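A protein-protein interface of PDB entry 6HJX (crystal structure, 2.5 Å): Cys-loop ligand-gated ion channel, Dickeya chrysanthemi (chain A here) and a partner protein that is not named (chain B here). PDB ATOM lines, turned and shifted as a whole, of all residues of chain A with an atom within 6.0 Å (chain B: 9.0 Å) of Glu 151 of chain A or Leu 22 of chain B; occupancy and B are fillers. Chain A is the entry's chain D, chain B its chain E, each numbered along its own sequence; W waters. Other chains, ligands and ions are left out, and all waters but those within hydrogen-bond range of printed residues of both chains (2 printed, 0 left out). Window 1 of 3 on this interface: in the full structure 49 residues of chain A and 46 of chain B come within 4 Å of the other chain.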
ATOM      1  N   LYS A  14       3.101 -20.117 -27.157  1.00  0.00           N
ATOM      2  CA  LYS A  14       4.201 -20.954 -26.699  1.00  0.00           C
ATOM      3  C   LYS A  14       5.371 -20.836 -27.665  1.00  0.00           C
ATOM      4  O   LYS A  14       5.179 -20.821 -28.884  1.00  0.00           O
ATOM      5  CB  LYS A  14       3.737 -22.412 -26.586  1.00  0.00           C
ATOM      6  CG  LYS A  14       4.603 -23.321 -25.729  1.00  0.00           C
ATOM      7  CD  LYS A  14       4.012 -24.731 -25.689  1.00  0.00           C
ATOM      8  CE  LYS A  14       4.944 -25.732 -25.007  1.00  0.00           C
ATOM      9  NZ  LYS A  14       5.104 -25.466 -23.556  1.00  0.00           N
ATOM     10  N   TYR A  16       9.093 -22.893 -27.918  1.00  0.00           N
ATOM     11  CA  TYR A  16       9.753 -24.053 -27.331  1.00  0.00           C
ATOM     12  C   TYR A  16      10.468 -24.820 -28.439  1.00  0.00           C
ATOM     13  O   TYR A  16      10.466 -24.418 -29.605  1.00  0.00           O
ATOM     14  CB  TYR A  16       8.736 -24.948 -26.613  1.00  0.00           C
ATOM     15  CG  TYR A  16       7.755 -25.594 -27.570  1.00  0.00           C
ATOM     16  CD1 TYR A  16       6.748 -24.848 -28.174  1.00  0.00           C
ATOM     17  CD2 TYR A  16       7.848 -26.943 -27.888  1.00  0.00           C
ATOM     18  CE1 TYR A  16       5.859 -25.429 -29.057  1.00  0.00           C
ATOM     19  CE2 TYR A  16       6.961 -27.533 -28.769  1.00  0.00           C
ATOM     20  CZ  TYR A  16       5.969 -26.769 -29.351  1.00  0.00           C
ATOM     21  OH  TYR A  16       5.087 -27.347 -30.231  1.00  0.00           O
ATOM     22  N   GLY A  17      11.080 -25.939 -28.062  1.00  0.00           N
ATOM     23  CA  GLY A  17      11.671 -26.841 -29.036  1.00  0.00           C
ATOM     24  C   GLY A  17      12.838 -26.264 -29.804  1.00  0.00           C
ATOM     25  O   GLY A  17      12.937 -26.467 -31.022  1.00  0.00           O
ATOM     26  N   GLU A 147       8.402 -17.893 -13.455  1.00  0.00           N
ATOM     27  CA  GLU A 147       9.294 -18.398 -14.491  1.00  0.00           C
ATOM     28  C   GLU A 147      10.351 -19.362 -13.963  1.00  0.00           C
ATOM     29  O   GLU A 147      11.140 -19.883 -14.759  1.00  0.00           O
ATOM     30  CB  GLU A 147       9.978 -17.226 -15.203  1.00  0.00           C
ATOM     31  CG  GLU A 147      10.857 -16.365 -14.302  1.00  0.00           C
ATOM     32  CD  GLU A 147      11.392 -15.137 -15.015  1.00  0.00           C
ATOM     33  OE1 GLU A 147      10.879 -14.807 -16.106  1.00  0.00           O
ATOM     34  OE2 GLU A 147      12.328 -14.501 -14.485  1.00  0.00           O
ATOM     35  N   ILE A 149      10.100 -22.320 -13.159  1.00  0.00           N
ATOM     36  CA  ILE A 149       9.926 -23.641 -13.754  1.00  0.00           C
ATOM     37  C   ILE A 149      10.100 -23.632 -15.267  1.00  0.00           C
ATOM     38  O   ILE A 149       9.936 -24.683 -15.906  1.00  0.00           O
ATOM     39  CB  ILE A 149       8.539 -24.229 -13.414  1.00  0.00           C
ATOM     40  CG1 ILE A 149       7.420 -23.362 -13.999  1.00  0.00           C
ATOM     41  CG2 ILE A 149       8.368 -24.357 -11.906  1.00  0.00           C
ATOM     42  CD1 ILE A 149       6.111 -24.107 -14.190  1.00  0.00           C
ATOM     43  N   ASP A 150      10.420 -22.486 -15.861  1.00  0.00           N
ATOM     44  CA  ASP A 150      10.495 -22.351 -17.309  1.00  0.00           C
ATOM     45  C   ASP A 150      11.942 -22.391 -17.783  1.00  0.00           C
ATOM     46  O   ASP A 150      12.865 -21.995 -17.066  1.00  0.00           O
ATOM     47  CB  ASP A 150       9.837 -21.048 -17.767  1.00  0.00           C
ATOM     48  CG  ASP A 150       8.350 -21.025 -17.496  1.00  0.00           C
ATOM     49  OD1 ASP A 150       7.724 -22.108 -17.510  1.00  0.00           O
ATOM     50  OD2 ASP A 150       7.806 -19.925 -17.267  1.00  0.00           O
ATOM     51  N   GLU A 151      12.128 -22.878 -19.010  1.00  0.00           N
ATOM     52  CA  GLU A 151      13.466 -22.990 -19.575  1.00  0.00           C
ATOM     53  C   GLU A 151      14.014 -21.644 -20.028  1.00  0.00           C
ATOM     54  O   GLU A 151      15.226 -21.420 -19.955  1.00  0.00           O
ATOM     55  CB  GLU A 151      13.459 -23.964 -20.754  1.00  0.00           C
ATOM     56  CG  GLU A 151      14.831 -24.221 -21.350  1.00  0.00           C
ATOM     57  CD  GLU A 151      14.803 -25.279 -22.432  1.00  0.00           C
ATOM     58  OE1 GLU A 151      13.697 -25.745 -22.781  1.00  0.00           O
ATOM     59  OE2 GLU A 151      15.887 -25.644 -22.933  1.00  0.00           O
ATOM     60  N   TRP A 152      13.148 -20.750 -20.499  1.00  0.00           N
ATOM     61  CA  TRP A 152      13.552 -19.437 -20.979  1.00  0.00           C
ATOM     62  C   TRP A 152      12.816 -18.359 -20.197  1.00  0.00           C
ATOM     63  O   TRP A 152      11.635 -18.512 -19.871  1.00  0.00           O
ATOM     64  CB  TRP A 152      13.270 -19.286 -22.479  1.00  0.00           C
ATOM     65  CG  TRP A 152      14.108 -20.188 -23.326  1.00  0.00           C
ATOM     66  CD1 TRP A 152      13.765 -21.420 -23.806  1.00  0.00           C
ATOM     67  CD2 TRP A 152      15.441 -19.935 -23.788  1.00  0.00           C
ATOM     68  NE1 TRP A 152      14.800 -21.947 -24.541  1.00  0.00           N
ATOM     69  CE2 TRP A 152      15.839 -21.054 -24.547  1.00  0.00           C
ATOM     70  CE3 TRP A 152      16.333 -18.869 -23.636  1.00  0.00           C
ATOM     71  CZ2 TRP A 152      17.092 -21.137 -25.150  1.00  0.00           C
ATOM     72  CZ3 TRP A 152      17.575 -18.954 -24.236  1.00  0.00           C
ATOM     73  CH2 TRP A 152      17.944 -20.081 -24.983  1.00  0.00           C
ATOM     74  N   TRP A 153      13.521 -17.271 -19.901  1.00  0.00           N
ATOM     75  CA  TRP A 153      12.976 -16.153 -19.138  1.00  0.00           C
ATOM     76  C   TRP A 153      12.743 -14.988 -20.093  1.00  0.00           C
ATOM     77  O   TRP A 153      13.700 -14.397 -20.605  1.00  0.00           O
ATOM     78  CB  TRP A 153      13.922 -15.763 -18.002  1.00  0.00           C
ATOM     79  CG  TRP A 153      14.071 -16.833 -16.953  1.00  0.00           C
ATOM     80  CD1 TRP A 153      13.280 -17.932 -16.787  1.00  0.00           C
ATOM     81  CD2 TRP A 153      15.074 -16.903 -15.932  1.00  0.00           C
ATOM     82  NE1 TRP A 153      13.726 -18.681 -15.727  1.00  0.00           N
ATOM     83  CE2 TRP A 153      14.826 -18.072 -15.184  1.00  0.00           C
ATOM     84  CE3 TRP A 153      16.156 -16.093 -15.576  1.00  0.00           C
ATOM     85  CZ2 TRP A 153      15.618 -18.449 -14.104  1.00  0.00           C
ATOM     86  CZ3 TRP A 153      16.943 -16.472 -14.505  1.00  0.00           C
ATOM     87  CH2 TRP A 153      16.670 -17.639 -13.782  1.00  0.00           C
ATOM     88  N   VAL A 190      16.157 -14.907 -21.979  1.00  0.00           N
ATOM     89  CA  VAL A 190      17.442 -15.313 -21.425  1.00  0.00           C
ATOM     90  C   VAL A 190      17.296 -16.734 -20.903  1.00  0.00           C
ATOM     91  O   VAL A 190      16.241 -17.103 -20.374  1.00  0.00           O
ATOM     92  CB  VAL A 190      17.907 -14.365 -20.300  1.00  0.00           C
ATOM     93  CG1 VAL A 190      19.316 -14.721 -19.855  1.00  0.00           C
ATOM     94  CG2 VAL A 190      17.836 -12.915 -20.757  1.00  0.00           C
ATOM     95  N   ARG A 191      18.347 -17.533 -21.057  1.00  0.00           N
ATOM     96  CA  ARG A 191      18.273 -18.928 -20.647  1.00  0.00           C
ATOM     97  C   ARG A 191      18.252 -19.036 -19.128  1.00  0.00           C
ATOM     98  O   ARG A 191      18.949 -18.299 -18.426  1.00  0.00           O
ATOM     99  CB  ARG A 191      19.454 -19.720 -21.210  1.00  0.00           C
ATOM    100  CG  ARG A 191      19.346 -21.223 -20.965  1.00  0.00           C
ATOM    101  CD  ARG A 191      20.563 -21.978 -21.468  1.00  0.00           C
ATOM    102  NE  ARG A 191      20.735 -21.851 -22.913  1.00  0.00           N
ATOM    103  CZ  ARG A 191      20.170 -22.649 -23.816  1.00  0.00           C
ATOM    104  NH1 ARG A 191      19.380 -23.648 -23.439  1.00  0.00           N
ATOM    105  NH2 ARG A 191      20.394 -22.445 -25.106  1.00  0.00           N
ATOM    106  N   ASN A 192      17.436 -19.958 -18.621  1.00  0.00           N
ATOM    107  CA  ASN A 192      17.437 -20.272 -17.198  1.00  0.00           C
ATOM    108  C   ASN A 192      18.671 -21.113 -16.890  1.00  0.00           C
ATOM    109  O   ASN A 192      18.726 -22.288 -17.274  1.00  0.00           O
ATOM    110  CB  ASN A 192      16.155 -21.010 -16.808  1.00  0.00           C
ATOM    111  CG  ASN A 192      16.121 -21.386 -15.336  1.00  0.00           C
ATOM    112  OD1 ASN A 192      17.029 -21.052 -14.573  1.00  0.00           O
ATOM    113  ND2 ASN A 192      15.062 -22.078 -14.927  1.00  0.00           N
ATOM    114  N   PRO A 193      19.677 -20.564 -16.205  1.00  0.00           N
ATOM    115  CA  PRO A 193      20.949 -21.276 -16.034  1.00  0.00           C
ATOM    116  C   PRO A 193      21.065 -22.110 -14.768  1.00  0.00           C
ATOM    117  O   PRO A 193      22.107 -22.747 -14.574  1.00  0.00           O
ATOM    118  CB  PRO A 193      21.951 -20.114 -15.997  1.00  0.00           C
ATOM    119  CG  PRO A 193      21.205 -19.047 -15.250  1.00  0.00           C
ATOM    120  CD  PRO A 193      19.726 -19.233 -15.569  1.00  0.00           C
ATOM    121  N   TYR A 196      22.275 -25.786 -15.125  1.00  0.00           N
ATOM    122  CA  TYR A 196      23.627 -25.866 -15.670  1.00  0.00           C
ATOM    123  C   TYR A 196      24.662 -25.327 -14.692  1.00  0.00           C
ATOM    124  O   TYR A 196      25.821 -25.758 -14.716  1.00  0.00           O
ATOM    125  CB  TYR A 196      23.705 -25.106 -16.996  1.00  0.00           C
ATOM    126  CG  TYR A 196      22.770 -25.651 -18.047  1.00  0.00           C
ATOM    127  CD1 TYR A 196      22.995 -26.893 -18.624  1.00  0.00           C
ATOM    128  CD2 TYR A 196      21.659 -24.929 -18.458  1.00  0.00           C
ATOM    129  CE1 TYR A 196      22.138 -27.402 -19.578  1.00  0.00           C
ATOM    130  CE2 TYR A 196      20.797 -25.428 -19.414  1.00  0.00           C
ATOM    131  CZ  TYR A 196      21.041 -26.665 -19.972  1.00  0.00           C
ATOM    132  OH  TYR A 196      20.189 -27.170 -20.927  1.00  0.00           O
ATOM    133  N   GLY B  18       3.174 -40.160 -22.796  1.00  0.00           N
ATOM    134  CA  GLY B  18       4.120 -39.406 -23.601  1.00  0.00           C
ATOM    135  C   GLY B  18       4.484 -38.055 -23.031  1.00  0.00           C
ATOM    136  O   GLY B  18       4.701 -37.101 -23.791  1.00  0.00           O
ATOM    137  N   VAL B  19       4.558 -37.941 -21.704  1.00  0.00           N
ATOM    138  CA  VAL B  19       4.963 -36.684 -21.093  1.00  0.00           C
ATOM    139  C   VAL B  19       6.319 -36.270 -21.644  1.00  0.00           C
ATOM    140  O   VAL B  19       7.242 -37.088 -21.755  1.00  0.00           O
ATOM    141  CB  VAL B  19       4.997 -36.813 -19.562  1.00  0.00           C
ATOM    142  CG1 VAL B  19       5.611 -35.568 -18.933  1.00  0.00           C
ATOM    143  CG2 VAL B  19       3.596 -37.047 -19.014  1.00  0.00           C
ATOM    144  N   ASN B  20       6.440 -34.996 -22.005  1.00  0.00           N
ATOM    145  CA  ASN B  20       7.713 -34.395 -22.390  1.00  0.00           C
ATOM    146  C   ASN B  20       8.023 -33.316 -21.362  1.00  0.00           C
ATOM    147  O   ASN B  20       7.401 -32.247 -21.371  1.00  0.00           O
ATOM    148  CB  ASN B  20       7.652 -33.823 -23.803  1.00  0.00           C
ATOM    149  CG  ASN B  20       9.000 -33.338 -24.293  1.00  0.00           C
ATOM    150  OD1 ASN B  20       9.788 -32.786 -23.529  1.00  0.00           O
ATOM    151  ND2 ASN B  20       9.272 -33.540 -25.576  1.00  0.00           N
ATOM    152  N   THR B  21       8.977 -33.597 -20.473  1.00  0.00           N
ATOM    153  CA  THR B  21       9.188 -32.727 -19.319  1.00  0.00           C
ATOM    154  C   THR B  21       9.645 -31.339 -19.750  1.00  0.00           C
ATOM    155  O   THR B  21       9.124 -30.326 -19.270  1.00  0.00           O
ATOM    156  CB  THR B  21      10.198 -33.361 -18.360  1.00  0.00           C
ATOM    157  OG1 THR B  21      11.347 -33.809 -19.091  1.00  0.00           O
ATOM    158  CG2 THR B  21       9.561 -34.535 -17.619  1.00  0.00           C
ATOM    159  N   LEU B  22      10.604 -31.269 -20.670  1.00  0.00           N
ATOM    160  CA  LEU B  22      11.159 -29.975 -21.045  1.00  0.00           C
ATOM    161  C   LEU B  22      10.145 -29.137 -21.813  1.00  0.00           C
ATOM    162  O   LEU B  22      10.097 -27.912 -21.650  1.00  0.00           O
ATOM    163  CB  LEU B  22      12.432 -30.168 -21.868  1.00  0.00           C
ATOM    164  CG  LEU B  22      13.288 -28.911 -22.043  1.00  0.00           C
ATOM    165  CD1 LEU B  22      13.869 -28.460 -20.710  1.00  0.00           C
ATOM    166  CD2 LEU B  22      14.395 -29.144 -23.057  1.00  0.00           C
ATOM    167  N   GLU B  23       9.328 -29.769 -22.655  1.00  0.00           N
ATOM    168  CA  GLU B  23       8.304 -29.051 -23.402  1.00  0.00           C
ATOM    169  C   GLU B  23       7.009 -28.883 -22.619  1.00  0.00           C
ATOM    170  O   GLU B  23       6.122 -28.154 -23.073  1.00  0.00           O
ATOM    171  CB  GLU B  23       8.015 -29.765 -24.726  1.00  0.00           C
ATOM    172  CG  GLU B  23       9.168 -29.699 -25.719  1.00  0.00           C
ATOM    173  CD  GLU B  23       8.844 -30.346 -27.051  1.00  0.00           C
ATOM    174  OE1 GLU B  23       7.704 -30.829 -27.220  1.00  0.00           O
ATOM    175  OE2 GLU B  23       9.731 -30.374 -27.932  1.00  0.00           O
ATOM    176  N   GLN B  24       6.894 -29.517 -21.454  1.00  0.00           N
ATOM    177  CA  GLN B  24       5.693 -29.436 -20.627  1.00  0.00           C
ATOM    178  C   GLN B  24       4.460 -29.806 -21.444  1.00  0.00           C
ATOM    179  O   GLN B  24       3.441 -29.111 -21.446  1.00  0.00           O
ATOM    180  CB  GLN B  24       5.557 -28.048 -19.999  1.00  0.00           C
ATOM    181  CG  GLN B  24       6.666 -27.728 -18.987  1.00  0.00           C
ATOM    182  CD  GLN B  24       6.555 -26.332 -18.404  1.00  0.00           C
ATOM    183  OE1 GLN B  24       5.458 -25.809 -18.213  1.00  0.00           O
ATOM    184  NE2 GLN B  24       7.697 -25.721 -18.122  1.00  0.00           N
ATOM    185  N   THR B  25       4.565 -30.928 -22.149  1.00  0.00           N
ATOM    186  CA  THR B  25       3.478 -31.443 -22.961  1.00  0.00           C
ATOM    187  C   THR B  25       3.202 -32.893 -22.585  1.00  0.00           C
ATOM    188  O   THR B  25       3.987 -33.550 -21.896  1.00  0.00           O
ATOM    189  CB  THR B  25       3.790 -31.339 -24.463  1.00  0.00           C
ATOM    190  OG1 THR B  25       5.040 -31.976 -24.742  1.00  0.00           O
ATOM    191  CG2 THR B  25       3.858 -29.887 -24.901  1.00  0.00           C
ATOM    192  N   ASN B 105       0.588 -27.614 -20.598  1.00  0.00           N
ATOM    193  CA  ASN B 105       0.096 -27.224 -19.285  1.00  0.00           C
ATOM    194  C   ASN B 105       1.298 -26.919 -18.405  1.00  0.00           C
ATOM    195  O   ASN B 105       2.362 -27.519 -18.581  1.00  0.00           O
ATOM    196  CB  ASN B 105      -0.759 -28.343 -18.676  1.00  0.00           C
ATOM    197  CG  ASN B 105      -1.687 -27.850 -17.594  1.00  0.00           C
ATOM    198  OD1 ASN B 105      -2.009 -26.664 -17.528  1.00  0.00           O
ATOM    199  ND2 ASN B 105      -2.132 -28.761 -16.741  1.00  0.00           N
ATOM    200  N   MET B 107       3.682 -27.486 -15.802  1.00  0.00           N
ATOM    201  CA  MET B 107       4.076 -28.693 -15.089  1.00  0.00           C
ATOM    202  C   MET B 107       5.377 -28.440 -14.348  1.00  0.00           C
ATOM    203  O   MET B 107       6.370 -28.023 -14.951  1.00  0.00           O
ATOM    204  CB  MET B 107       4.230 -29.879 -16.045  1.00  0.00           C
ATOM    205  CG  MET B 107       2.935 -30.268 -16.725  1.00  0.00           C
ATOM    206  SD  MET B 107       2.929 -31.973 -17.304  1.00  0.00           S
ATOM    207  CE  MET B 107       3.889 -31.818 -18.801  1.00  0.00           C
ATOM    208  N   PHE B 109       8.239 -30.182 -12.239  1.00  0.00           N
ATOM    209  CA  PHE B 109       8.888 -31.449 -11.928  1.00  0.00           C
ATOM    210  C   PHE B 109       9.992 -31.301 -10.882  1.00  0.00           C
ATOM    211  O   PHE B 109      10.884 -32.151 -10.811  1.00  0.00           O
ATOM    212  CB  PHE B 109       9.463 -32.075 -13.202  1.00  0.00           C
ATOM    213  CG  PHE B 109       8.473 -32.180 -14.333  1.00  0.00           C
ATOM    214  CD1 PHE B 109       7.554 -33.218 -14.377  1.00  0.00           C
ATOM    215  CD2 PHE B 109       8.468 -31.245 -15.358  1.00  0.00           C
ATOM    216  CE1 PHE B 109       6.646 -33.319 -15.415  1.00  0.00           C
ATOM    217  CE2 PHE B 109       7.562 -31.339 -16.400  1.00  0.00           C
ATOM    218  CZ  PHE B 109       6.649 -32.379 -16.429  1.00  0.00           C
ATOM    219  N   PRO B 247      14.665 -37.460 -16.807  1.00  0.00           N
ATOM    220  CA  PRO B 247      14.210 -36.498 -17.814  1.00  0.00           C
ATOM    221  C   PRO B 247      15.024 -35.216 -17.782  1.00  0.00           C
ATOM    222  O   PRO B 247      15.637 -34.855 -16.775  1.00  0.00           O
ATOM    223  CB  PRO B 247      12.750 -36.241 -17.426  1.00  0.00           C
ATOM    224  CG  PRO B 247      12.716 -36.473 -15.955  1.00  0.00           C
ATOM    225  CD  PRO B 247      13.708 -37.582 -15.690  1.00  0.00           C
ATOM    226  N   ARG B 248      15.019 -34.524 -18.918  1.00  0.00           N
ATOM    227  CA  ARG B 248      15.702 -33.244 -19.041  1.00  0.00           C
ATOM    228  C   ARG B 248      14.817 -32.127 -18.502  1.00  0.00           C
ATOM    229  O   ARG B 248      13.638 -32.030 -18.857  1.00  0.00           O
ATOM    230  CB  ARG B 248      16.066 -32.976 -20.500  1.00  0.00           C
ATOM    231  CG  ARG B 248      17.142 -33.904 -21.048  1.00  0.00           C
ATOM    232  CD  ARG B 248      18.492 -33.685 -20.373  1.00  0.00           C
ATOM    233  NE  ARG B 248      18.888 -32.278 -20.395  1.00  0.00           N
ATOM    234  CZ  ARG B 248      18.953 -31.482 -19.328  1.00  0.00           C
ATOM    235  NH1 ARG B 248      18.667 -31.936 -18.111  1.00  0.00           N
ATOM    236  NH2 ARG B 248      19.319 -30.216 -19.480  1.00  0.00           N
ATOM    237  N   LEU B 249      15.386 -31.287 -17.650  1.00  0.00           N
ATOM    238  CA  LEU B 249      14.657 -30.221 -16.975  1.00  0.00           C
ATOM    239  C   LEU B 249      15.526 -28.996 -16.909  1.00  0.00           C
ATOM    240  O   LEU B 249      16.760 -29.073 -16.982  1.00  0.00           O
ATOM    241  CB  LEU B 249      14.244 -30.643 -15.557  1.00  0.00           C
ATOM    242  CG  LEU B 249      13.232 -31.783 -15.472  1.00  0.00           C
ATOM    243  CD1 LEU B 249      13.264 -32.427 -14.095  1.00  0.00           C
ATOM    244  CD2 LEU B 249      11.839 -31.270 -15.799  1.00  0.00           C
ATOM    245  N   PRO B 250      14.926 -27.798 -16.770  1.00  0.00           N
ATOM    246  CA  PRO B 250      15.701 -26.574 -16.580  1.00  0.00           C
ATOM    247  C   PRO B 250      16.088 -26.277 -15.135  1.00  0.00           C
ATOM    248  O   PRO B 250      16.530 -25.158 -14.856  1.00  0.00           O
ATOM    249  CB  PRO B 250      14.744 -25.495 -17.106  1.00  0.00           C
ATOM    250  CG  PRO B 250      13.388 -26.031 -16.826  1.00  0.00           C
ATOM    251  CD  PRO B 250      13.480 -27.534 -16.909  1.00  0.00           C
ATOM    252  N   TYR B 251      15.930 -27.238 -14.227  1.00  0.00           N
ATOM    253  CA  TYR B 251      16.262 -27.053 -12.823  1.00  0.00           C
ATOM    254  C   TYR B 251      16.722 -28.386 -12.251  1.00  0.00           C
ATOM    255  O   TYR B 251      16.496 -29.446 -12.841  1.00  0.00           O
ATOM    256  CB  TYR B 251      15.066 -26.508 -12.031  1.00  0.00           C
ATOM    257  CG  TYR B 251      13.742 -27.105 -12.448  1.00  0.00           C
ATOM    258  CD1 TYR B 251      13.338 -28.351 -11.984  1.00  0.00           C
ATOM    259  CD2 TYR B 251      12.896 -26.423 -13.311  1.00  0.00           C
ATOM    260  CE1 TYR B 251      12.132 -28.900 -12.368  1.00  0.00           C
ATOM    261  CE2 TYR B 251      11.683 -26.965 -13.701  1.00  0.00           C
ATOM    262  CZ  TYR B 251      11.308 -28.204 -13.225  1.00  0.00           C
ATOM    263  OH  TYR B 251      10.107 -28.753 -13.607  1.00  0.00           O
HETATM  264  O   HOH W   1       9.189 -27.442 -15.612  1.00  0.00           O
HETATM  265  O   HOH W   2       3.619 -25.525 -21.025  1.00  0.00           O
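Printed residues of chain B within 4 Å of Lys 14 of chain A: Glu 23. Printed residues of chain B within 4 Å of Asn 192 of chain A: Pro 250. Leu 22 of chain B touches just one residue of chain A: Glu 151. Of the printed residues of chain A, Glu 23 of chain B touches Lys 14 and Tyr 16. Of the printed residues of chain A, Met 107 of chain B touches Ile 149 (3.998 Å). Of the printed residues of chain A, Pro 250 of chain B touches Ile 149, Asp 150, Glu 151 and Asn 192. The nearest residue of chain B that does not touch Glu 151 of chain A is Gln 24 of chain B (5.3 Å).
NE2 of Gln 24 of chain B lies within hydrogen-bond range of O of Ile 149 of chain A. OH of Tyr 196 of chain A is in hydrogen-bond range of NH2 of Arg 248 of chain B (3.5 Å). The backbone carbonyl oxygen (O) of Glu 23 of chain B is in hydrogen-bond range of the side-chain amino group (NZ) of Lys 14 of chain A, at 2.9 Å. The side-chain amide nitrogen (ND2) of Asn 192 of chain A sits at hydrogen-bond distance from the backbone carbonyl oxygen (O) of Pro 250 of chain B.
The backbone carbonyl oxygen (O) of Asp 150 of chain A lies within hydrogen-bond range of the side-chain amide nitrogen (ND2) of Asn 192 of chain A (3.1 Å). N of Asn 192 of chain A is in hydrogen-bond range of O of Glu 151 of chain A (3.0 Å). The backbone NH (N) of Glu 23 of chain B is in hydrogen-bond range of the side-chain amide oxygen (OD1) of Asn 20 of chain B (3.2 Å). The backbone NH (N) of Asn 105 of chain B lies within hydrogen-bond range of the backbone carbonyl oxygen (O) of Gln 24 of chain B, 3.3 Å away. The side-chain hydroxyl (OG1) of Thr 21 of chain B sits at hydrogen-bond distance from the backbone carbonyl oxygen (O) of Arg 248 of chain B (2.9 Å). N of Phe 109 of chain B is in hydrogen-bond range of OH of Tyr 251 of chain B (2.7 Å).
Water W1 lies within hydrogen-bond range of OH of Tyr 251 of chain B (2.6 Å), O of Ile 149 of chain A (2.9 Å), O of Met 107 of chain B (3.0 Å) and NE2 of Gln 24 of chain B (3.4 Å). Water W2 lies within hydrogen-bond range of the side-chain amino group (NZ) of Lys 14 of chain A (2.9 Å), the side-chain amide oxygen (OE1) of Gln 24 of chain B (3.4 Å) and the backbone carbonyl oxygen (O) of Asn 105 of chain B (3.4 Å).
Glu 23 of chain B touches Tyr 16 of chain A (CD to CD2, 3.6 Å). Ile 149 of chain A touches Met 107 of chain B. Pro 250 of chain B touches Ile 149 of chain A. Ile 149 of chain A touches Tyr 251 of chain B. Asp 150 of chain A touches Gln 24 of chain B. Pro 250 of chain B touches Asp 150 of chain A (CB to O, 3.97 Å). OE1 of Glu 151 of chain A touches CG of Leu 22 of chain B, at 3.3 Å. Glu 151 of chain A touches Pro 250 of chain B (CA to CB, 3.7 Å).
Printed residues of chain A that touch a printed residue of chain B: Lys 14, Tyr 16, Ile 149, Asp 150, Glu 151, Asn 192 and Tyr 196. Hydrophobic or aromatic side chains of chain A that line the printed part of chain B: Tyr 16, Ile 149 and Tyr 196. Along chain A the printed residues that touch a printed residue of chain B span positions 14 to 196. Of the 16 printed residues of chain B, 7 touch a printed residue of chain A. Hydrophobic or aromatic side chains of chain B within 4 Å of the printed part of chain A: Leu 22, Pro 250 and Tyr 251.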
